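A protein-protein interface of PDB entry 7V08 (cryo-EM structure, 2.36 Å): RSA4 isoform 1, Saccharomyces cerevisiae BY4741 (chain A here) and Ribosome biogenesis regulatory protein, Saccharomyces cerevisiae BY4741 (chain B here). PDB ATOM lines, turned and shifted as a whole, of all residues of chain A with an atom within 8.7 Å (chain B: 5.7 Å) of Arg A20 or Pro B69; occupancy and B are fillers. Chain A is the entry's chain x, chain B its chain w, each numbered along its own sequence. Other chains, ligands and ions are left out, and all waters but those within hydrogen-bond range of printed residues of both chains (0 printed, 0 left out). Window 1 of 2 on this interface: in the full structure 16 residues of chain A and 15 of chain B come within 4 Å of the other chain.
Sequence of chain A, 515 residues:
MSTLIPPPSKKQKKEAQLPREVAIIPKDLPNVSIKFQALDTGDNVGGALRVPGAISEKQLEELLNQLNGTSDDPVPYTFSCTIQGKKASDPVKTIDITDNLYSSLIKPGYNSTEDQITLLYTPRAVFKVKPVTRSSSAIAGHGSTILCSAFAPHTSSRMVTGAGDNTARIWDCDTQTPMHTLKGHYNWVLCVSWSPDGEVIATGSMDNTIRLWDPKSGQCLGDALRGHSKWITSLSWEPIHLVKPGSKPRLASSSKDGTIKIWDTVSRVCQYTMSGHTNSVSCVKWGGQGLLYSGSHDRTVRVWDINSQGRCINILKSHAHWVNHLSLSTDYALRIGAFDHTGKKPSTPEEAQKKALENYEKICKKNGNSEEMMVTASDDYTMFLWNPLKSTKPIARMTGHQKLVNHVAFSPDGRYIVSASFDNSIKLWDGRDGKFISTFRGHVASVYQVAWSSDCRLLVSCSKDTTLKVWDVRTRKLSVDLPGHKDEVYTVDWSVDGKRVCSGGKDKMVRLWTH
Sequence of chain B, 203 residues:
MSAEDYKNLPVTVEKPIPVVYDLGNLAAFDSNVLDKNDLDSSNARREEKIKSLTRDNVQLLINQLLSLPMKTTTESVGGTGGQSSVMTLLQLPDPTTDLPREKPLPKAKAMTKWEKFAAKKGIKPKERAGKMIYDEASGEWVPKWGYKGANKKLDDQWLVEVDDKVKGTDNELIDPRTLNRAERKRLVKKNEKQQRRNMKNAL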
ATOM      1  N   GLN A  12      -4.768 -10.007   6.627  1.00  0.00           N
ATOM      2  CA  GLN A  12      -5.385  -9.555   7.869  1.00  0.00           C
ATOM      3  C   GLN A  12      -4.479  -8.580   8.609  1.00  0.00           C
ATOM      4  O   GLN A  12      -4.957  -7.596   9.186  1.00  0.00           O
ATOM      5  CB  GLN A  12      -5.739 -10.762   8.742  1.00  0.00           C
ATOM      6  CG  GLN A  12      -6.606 -11.785   8.008  1.00  0.00           C
ATOM      7  CD  GLN A  12      -7.101 -12.924   8.884  1.00  0.00           C
ATOM      8  OE1 GLN A  12      -6.658 -13.100  10.018  1.00  0.00           O
ATOM      9  NE2 GLN A  12      -8.029 -13.707   8.350  1.00  0.00           N
ATOM     10  N   LYS A  14      -2.349  -6.587   7.094  1.00  0.00           N
ATOM     11  CA  LYS A  14      -2.442  -5.349   6.319  1.00  0.00           C
ATOM     12  C   LYS A  14      -3.709  -4.563   6.651  1.00  0.00           C
ATOM     13  O   LYS A  14      -3.670  -3.334   6.812  1.00  0.00           O
ATOM     14  CB  LYS A  14      -2.395  -5.660   4.823  1.00  0.00           C
ATOM     15  CG  LYS A  14      -1.005  -5.848   4.254  1.00  0.00           C
ATOM     16  CD  LYS A  14      -0.218  -4.548   4.258  1.00  0.00           C
ATOM     17  CE  LYS A  14      -0.980  -3.410   3.579  1.00  0.00           C
ATOM     18  NZ  LYS A  14      -1.140  -3.591   2.104  1.00  0.00           N
ATOM     19  N   GLU A  15      -4.847  -5.252   6.750  1.00  0.00           N
ATOM     20  CA  GLU A  15      -6.089  -4.561   7.081  1.00  0.00           C
ATOM     21  C   GLU A  15      -6.057  -4.034   8.511  1.00  0.00           C
ATOM     22  O   GLU A  15      -6.678  -3.008   8.816  1.00  0.00           O
ATOM     23  CB  GLU A  15      -7.287  -5.485   6.870  1.00  0.00           C
ATOM     24  CG  GLU A  15      -7.608  -5.746   5.411  1.00  0.00           C
ATOM     25  CD  GLU A  15      -8.946  -6.431   5.225  1.00  0.00           C
ATOM     26  OE1 GLU A  15      -9.742  -6.448   6.189  1.00  0.00           O
ATOM     27  OE2 GLU A  15      -9.198  -6.955   4.118  1.00  0.00           O
ATOM     28  N   ALA A  16      -5.352  -4.730   9.404  1.00  0.00           N
ATOM     29  CA  ALA A  16      -5.142  -4.214  10.750  1.00  0.00           C
ATOM     30  C   ALA A  16      -4.301  -2.945  10.729  1.00  0.00           C
ATOM     31  O   ALA A  16      -4.550  -2.012  11.501  1.00  0.00           O
ATOM     32  CB  ALA A  16      -4.479  -5.282  11.617  1.00  0.00           C
ATOM     33  N   GLN A  17      -3.289  -2.897   9.860  1.00  0.00           N
ATOM     34  CA  GLN A  17      -2.476  -1.691   9.734  1.00  0.00           C
ATOM     35  C   GLN A  17      -3.233  -0.538   9.083  1.00  0.00           C
ATOM     36  O   GLN A  17      -2.839   0.617   9.270  1.00  0.00           O
ATOM     37  CB  GLN A  17      -1.196  -1.991   8.953  1.00  0.00           C
ATOM     38  CG  GLN A  17      -0.168  -2.763   9.752  1.00  0.00           C
ATOM     39  CD  GLN A  17       1.123  -2.993   8.999  1.00  0.00           C
ATOM     40  OE1 GLN A  17       1.137  -3.101   7.774  1.00  0.00           O
ATOM     41  NE2 GLN A  17       2.221  -3.067   9.730  1.00  0.00           N
ATOM     42  N   LEU A  18      -4.291  -0.821   8.322  1.00  0.00           N
ATOM     43  CA  LEU A  18      -5.105   0.261   7.770  1.00  0.00           C
ATOM     44  C   LEU A  18      -5.719   1.092   8.900  1.00  0.00           C
ATOM     45  O   LEU A  18      -6.128   0.543   9.927  1.00  0.00           O
ATOM     46  CB  LEU A  18      -6.215  -0.284   6.873  1.00  0.00           C
ATOM     47  CG  LEU A  18      -5.848  -0.963   5.554  1.00  0.00           C
ATOM     48  CD1 LEU A  18      -7.081  -1.610   4.928  1.00  0.00           C
ATOM     49  CD2 LEU A  18      -5.209   0.020   4.593  1.00  0.00           C
ATOM     50  N   PRO A  19      -5.783   2.420   8.743  1.00  0.00           N
ATOM     51  CA  PRO A  19      -6.223   3.277   9.851  1.00  0.00           C
ATOM     52  C   PRO A  19      -7.664   3.007  10.258  1.00  0.00           C
ATOM     53  O   PRO A  19      -8.532   2.741   9.425  1.00  0.00           O
ATOM     54  CB  PRO A  19      -6.060   4.694   9.290  1.00  0.00           C
ATOM     55  CG  PRO A  19      -6.139   4.525   7.825  1.00  0.00           C
ATOM     56  CD  PRO A  19      -5.481   3.207   7.536  1.00  0.00           C
ATOM     57  N   ARG A  20      -7.906   3.096  11.561  1.00  0.00           N
ATOM     58  CA  ARG A  20      -9.165   2.695  12.170  1.00  0.00           C
ATOM     59  C   ARG A  20     -10.190   3.811  12.053  1.00  0.00           C
ATOM     60  O   ARG A  20      -9.842   4.992  11.981  1.00  0.00           O
ATOM     61  CB  ARG A  20      -8.973   2.336  13.647  1.00  0.00           C
ATOM     62  CG  ARG A  20      -7.769   1.450  13.945  1.00  0.00           C
ATOM     63  CD  ARG A  20      -8.059   0.002  13.609  1.00  0.00           C
ATOM     64  NE  ARG A  20      -9.371  -0.406  14.094  1.00  0.00           N
ATOM     65  CZ  ARG A  20      -9.856  -1.636  13.997  1.00  0.00           C
ATOM     66  NH1 ARG A  20      -9.154  -2.613  13.450  1.00  0.00           N
ATOM     67  NH2 ARG A  20     -11.075  -1.891  14.466  1.00  0.00           N
ATOM     68  N   GLU A  21     -11.461   3.424  12.027  1.00  0.00           N
ATOM     69  CA  GLU A  21     -12.539   4.399  12.037  1.00  0.00           C
ATOM     70  C   GLU A  21     -13.054   4.605  13.457  1.00  0.00           C
ATOM     71  O   GLU A  21     -13.091   3.677  14.271  1.00  0.00           O
ATOM     72  CB  GLU A  21     -13.674   3.957  11.111  1.00  0.00           C
ATOM     73  CG  GLU A  21     -14.356   2.661  11.514  1.00  0.00           C
ATOM     74  CD  GLU A  21     -15.393   2.196  10.507  1.00  0.00           C
ATOM     75  OE1 GLU A  21     -15.839   3.012   9.675  1.00  0.00           O
ATOM     76  OE2 GLU A  21     -15.757   1.001  10.539  1.00  0.00           O
ATOM     77  N   VAL A  22     -13.465   5.835  13.747  1.00  0.00           N
ATOM     78  CA  VAL A  22     -13.905   6.230  15.078  1.00  0.00           C
ATOM     79  C   VAL A  22     -15.425   6.288  15.082  1.00  0.00           C
ATOM     80  O   VAL A  22     -16.027   6.984  14.257  1.00  0.00           O
ATOM     81  CB  VAL A  22     -13.298   7.580  15.501  1.00  0.00           C
ATOM     82  CG1 VAL A  22     -13.924   8.079  16.798  1.00  0.00           C
ATOM     83  CG2 VAL A  22     -11.799   7.444  15.666  1.00  0.00           C
ATOM     84  N   ALA A  23     -16.039   5.553  16.006  1.00  0.00           N
ATOM     85  CA  ALA A  23     -17.493   5.524  16.147  1.00  0.00           C
ATOM     86  C   ALA A  23     -17.920   6.805  16.853  1.00  0.00           C
ATOM     87  O   ALA A  23     -17.912   6.899  18.081  1.00  0.00           O
ATOM     88  CB  ALA A  23     -17.938   4.284  16.910  1.00  0.00           C
ATOM     89  N   LEU B  23       0.416   2.827  14.636  1.00  0.00           N
ATOM     90  CA  LEU B  23      -0.099   2.389  15.925  1.00  0.00           C
ATOM     91  C   LEU B  23       0.751   1.300  16.567  1.00  0.00           C
ATOM     92  O   LEU B  23       0.574   1.017  17.755  1.00  0.00           O
ATOM     93  CB  LEU B  23      -1.541   1.904  15.771  1.00  0.00           C
ATOM     94  CG  LEU B  23      -2.564   2.946  15.315  1.00  0.00           C
ATOM     95  CD1 LEU B  23      -3.932   2.311  15.120  1.00  0.00           C
ATOM     96  CD2 LEU B  23      -2.648   4.102  16.302  1.00  0.00           C
ATOM     97  N   GLN B  64      -7.715   6.779  17.689  1.00  0.00           N
ATOM     98  CA  GLN B  64      -7.368   5.562  16.958  1.00  0.00           C
ATOM     99  C   GLN B  64      -7.085   4.392  17.897  1.00  0.00           C
ATOM    100  O   GLN B  64      -7.549   3.264  17.663  1.00  0.00           O
ATOM    101  CB  GLN B  64      -6.169   5.832  16.059  1.00  0.00           C
ATOM    102  CG  GLN B  64      -6.473   6.821  14.968  1.00  0.00           C
ATOM    103  CD  GLN B  64      -7.387   6.241  13.919  1.00  0.00           C
ATOM    104  OE1 GLN B  64      -7.306   5.058  13.603  1.00  0.00           O
ATOM    105  NE2 GLN B  64      -8.259   7.071  13.365  1.00  0.00           N
ATOM    106  N   SER B  67     -10.108   3.040  19.145  1.00  0.00           N
ATOM    107  CA  SER B  67     -10.795   2.333  18.071  1.00  0.00           C
ATOM    108  C   SER B  67     -10.168   0.984  17.739  1.00  0.00           C
ATOM    109  O   SER B  67     -10.755   0.225  16.961  1.00  0.00           O
ATOM    110  CB  SER B  67     -10.825   3.191  16.802  1.00  0.00           C
ATOM    111  OG  SER B  67     -11.484   4.420  17.034  1.00  0.00           O
ATOM    112  N   LEU B  68      -8.990   0.683  18.284  1.00  0.00           N
ATOM    113  CA  LEU B  68      -8.360  -0.612  18.044  1.00  0.00           C
ATOM    114  C   LEU B  68      -9.198  -1.759  18.617  1.00  0.00           C
ATOM    115  O   LEU B  68      -9.956  -1.570  19.569  1.00  0.00           O
ATOM    116  CB  LEU B  68      -6.971  -0.658  18.672  1.00  0.00           C
ATOM    117  CG  LEU B  68      -5.817  -0.022  17.912  1.00  0.00           C
ATOM    118  CD1 LEU B  68      -4.538  -0.160  18.717  1.00  0.00           C
ATOM    119  CD2 LEU B  68      -5.683  -0.668  16.549  1.00  0.00           C
ATOM    120  N   PRO B  69      -9.082  -2.956  18.043  1.00  0.00           N
ATOM    121  CA  PRO B  69      -9.697  -4.137  18.659  1.00  0.00           C
ATOM    122  C   PRO B  69      -9.011  -4.507  19.967  1.00  0.00           C
ATOM    123  O   PRO B  69      -7.837  -4.210  20.203  1.00  0.00           O
ATOM    124  CB  PRO B  69      -9.505  -5.229  17.602  1.00  0.00           C
ATOM    125  CG  PRO B  69      -8.348  -4.779  16.799  1.00  0.00           C
ATOM    126  CD  PRO B  69      -8.441  -3.285  16.757  1.00  0.00           C
ATOM    127  N   MET B  70      -9.777  -5.161  20.835  1.00  0.00           N
ATOM    128  CA  MET B  70      -9.355  -5.396  22.207  1.00  0.00           C
ATOM    129  C   MET B  70      -9.404  -6.879  22.547  1.00  0.00           C
ATOM    130  O   MET B  70     -10.318  -7.596  22.129  1.00  0.00           O
ATOM    131  CB  MET B  70     -10.225  -4.594  23.178  1.00  0.00           C
ATOM    132  CG  MET B  70     -10.382  -3.134  22.767  1.00  0.00           C
ATOM    133  SD  MET B  70     -10.801  -2.008  24.099  1.00  0.00           S
ATOM    134  CE  MET B  70     -10.891  -0.467  23.195  1.00  0.00           C
ATOM    135  N   LYS B  71      -8.414  -7.327  23.310  1.00  0.00           N
ATOM    136  CA  LYS B  71      -8.343  -8.696  23.794  1.00  0.00           C
ATOM    137  C   LYS B  71      -8.810  -8.744  25.241  1.00  0.00           C
ATOM    138  O   LYS B  71      -8.375  -7.934  26.073  1.00  0.00           O
ATOM    139  CB  LYS B  71      -6.925  -9.261  23.680  1.00  0.00           C
ATOM    140  CG  LYS B  71      -6.820 -10.729  24.070  1.00  0.00           C
ATOM    141  CD  LYS B  71      -5.409 -11.260  23.895  1.00  0.00           C
ATOM    142  CE  LYS B  71      -5.249 -12.637  24.530  1.00  0.00           C
ATOM    143  NZ  LYS B  71      -5.950 -13.714  23.778  1.00  0.00           N
ATOM    144  N   LEU B  89      -6.985  -5.524  27.160  1.00  0.00           N
ATOM    145  CA  LEU B  89      -5.813  -4.965  26.505  1.00  0.00           C
ATOM    146  C   LEU B  89      -6.152  -4.567  25.075  1.00  0.00           C
ATOM    147  O   LEU B  89      -7.114  -5.057  24.484  1.00  0.00           O
ATOM    148  CB  LEU B  89      -4.649  -5.964  26.514  1.00  0.00           C
ATOM    149  CG  LEU B  89      -4.174  -6.508  27.864  1.00  0.00           C
ATOM    150  CD1 LEU B  89      -3.117  -7.590  27.666  1.00  0.00           C
ATOM    151  CD2 LEU B  89      -3.638  -5.399  28.753  1.00  0.00           C
ATOM    152  N   LEU B  90      -5.358  -3.652  24.526  1.00  0.00           N
ATOM    153  CA  LEU B  90      -5.483  -3.261  23.128  1.00  0.00           C
ATOM    154  C   LEU B  90      -4.579  -4.131  22.270  1.00  0.00           C
ATOM    155  O   LEU B  90      -3.488  -4.512  22.691  1.00  0.00           O
ATOM    156  CB  LEU B  90      -5.103  -1.793  22.926  1.00  0.00           C
ATOM    157  CG  LEU B  90      -5.728  -0.709  23.807  1.00  0.00           C
ATOM    158  CD1 LEU B  90      -5.035   0.609  23.544  1.00  0.00           C
ATOM    159  CD2 LEU B  90      -7.217  -0.585  23.559  1.00  0.00           C
ATOM    160  N   GLN B  91      -5.026  -4.434  21.052  1.00  0.00           N
ATOM    161  CA  GLN B  91      -4.217  -5.191  20.099  1.00  0.00           C
ATOM    162  C   GLN B  91      -3.557  -4.202  19.145  1.00  0.00           C
ATOM    163  O   GLN B  91      -4.212  -3.633  18.270  1.00  0.00           O
ATOM    164  CB  GLN B  91      -5.068  -6.213  19.354  1.00  0.00           C
ATOM    165  CG  GLN B  91      -5.624  -7.302  20.243  1.00  0.00           C
ATOM    166  CD  GLN B  91      -6.165  -8.465  19.450  1.00  0.00           C
ATOM    167  OE1 GLN B  91      -6.865  -8.282  18.458  1.00  0.00           O
ATOM    168  NE2 GLN B  91      -5.837  -9.677  19.880  1.00  0.00           N
ATOM    169  N   LEU B  92      -2.266  -3.978  19.335  1.00  0.00           N
ATOM    170  CA  LEU B  92      -1.530  -3.057  18.479  1.00  0.00           C
ATOM    171  C   LEU B  92      -1.160  -3.748  17.173  1.00  0.00           C
ATOM    172  O   LEU B  92      -0.644  -4.870  17.199  1.00  0.00           O
ATOM    173  CB  LEU B  92      -0.270  -2.565  19.183  1.00  0.00           C
ATOM    174  CG  LEU B  92      -0.427  -1.925  20.560  1.00  0.00           C
ATOM    175  CD1 LEU B  92       0.919  -1.757  21.233  1.00  0.00           C
ATOM    176  CD2 LEU B  92      -1.146  -0.594  20.473  1.00  0.00           C
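Among the printed residues, merely in contact across the chains: Pro A19 with Gln B64, Arg A20 with Leu B68, Arg A20 with Pro B69 and Val A22 with Ser B67.
The side-chain amide oxygen (OE1) of Gln B64 lies within hydrogen-bond range of the backbone NH (N) of Arg A20, 2.9 Å away.
The guanidinium group (NE) of Arg A20 sits at hydrogen-bond distance from the backbone carbonyl oxygen (O) of Ser B67 (3.2 Å).
OG of Ser B67 is in hydrogen-bond range of O of Glu A21.
O of Pro B69 is in hydrogen-bond range of N of Gln B91, 2.9 Å away.
Of the 11 printed residues of chain A, 4 touch a printed residue of chain B.
Hydrophobic or aromatic side chains of chain A that line the printed part of chain B: Val A22.
Along chain A the printed residues that touch a printed residue of chain B span positions 19 to 22.
Among the printed residues, no Asp or Glu carboxylate lies within 4 Å of a Lys or Arg side-chain nitrogen of the other chain.
Gln A17 touches none of the printed residues of chain B.
Arg A20 touches just these residues of chain B: Gln B64, Ser B67, Leu B68 and Pro B69.
Of the printed residues of chain B, Val A22 touches Ser B67 (3.3 Å).
Printed residues of chain A within 4 Å of Ser B67: Arg A20 (3.2 Å), Glu A21 (3.3 Å) and Val A22 (3.3 Å).
Of the printed residues of chain A, Leu B68 touches Arg A20 (3.8 Å).
Pro B69 touches one residue of chain A.
Leu B92 touches none of the printed residues of chain A.
The nearest residue of chain A that does not touch Pro B69 is Ala A16 (6.5 Å).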
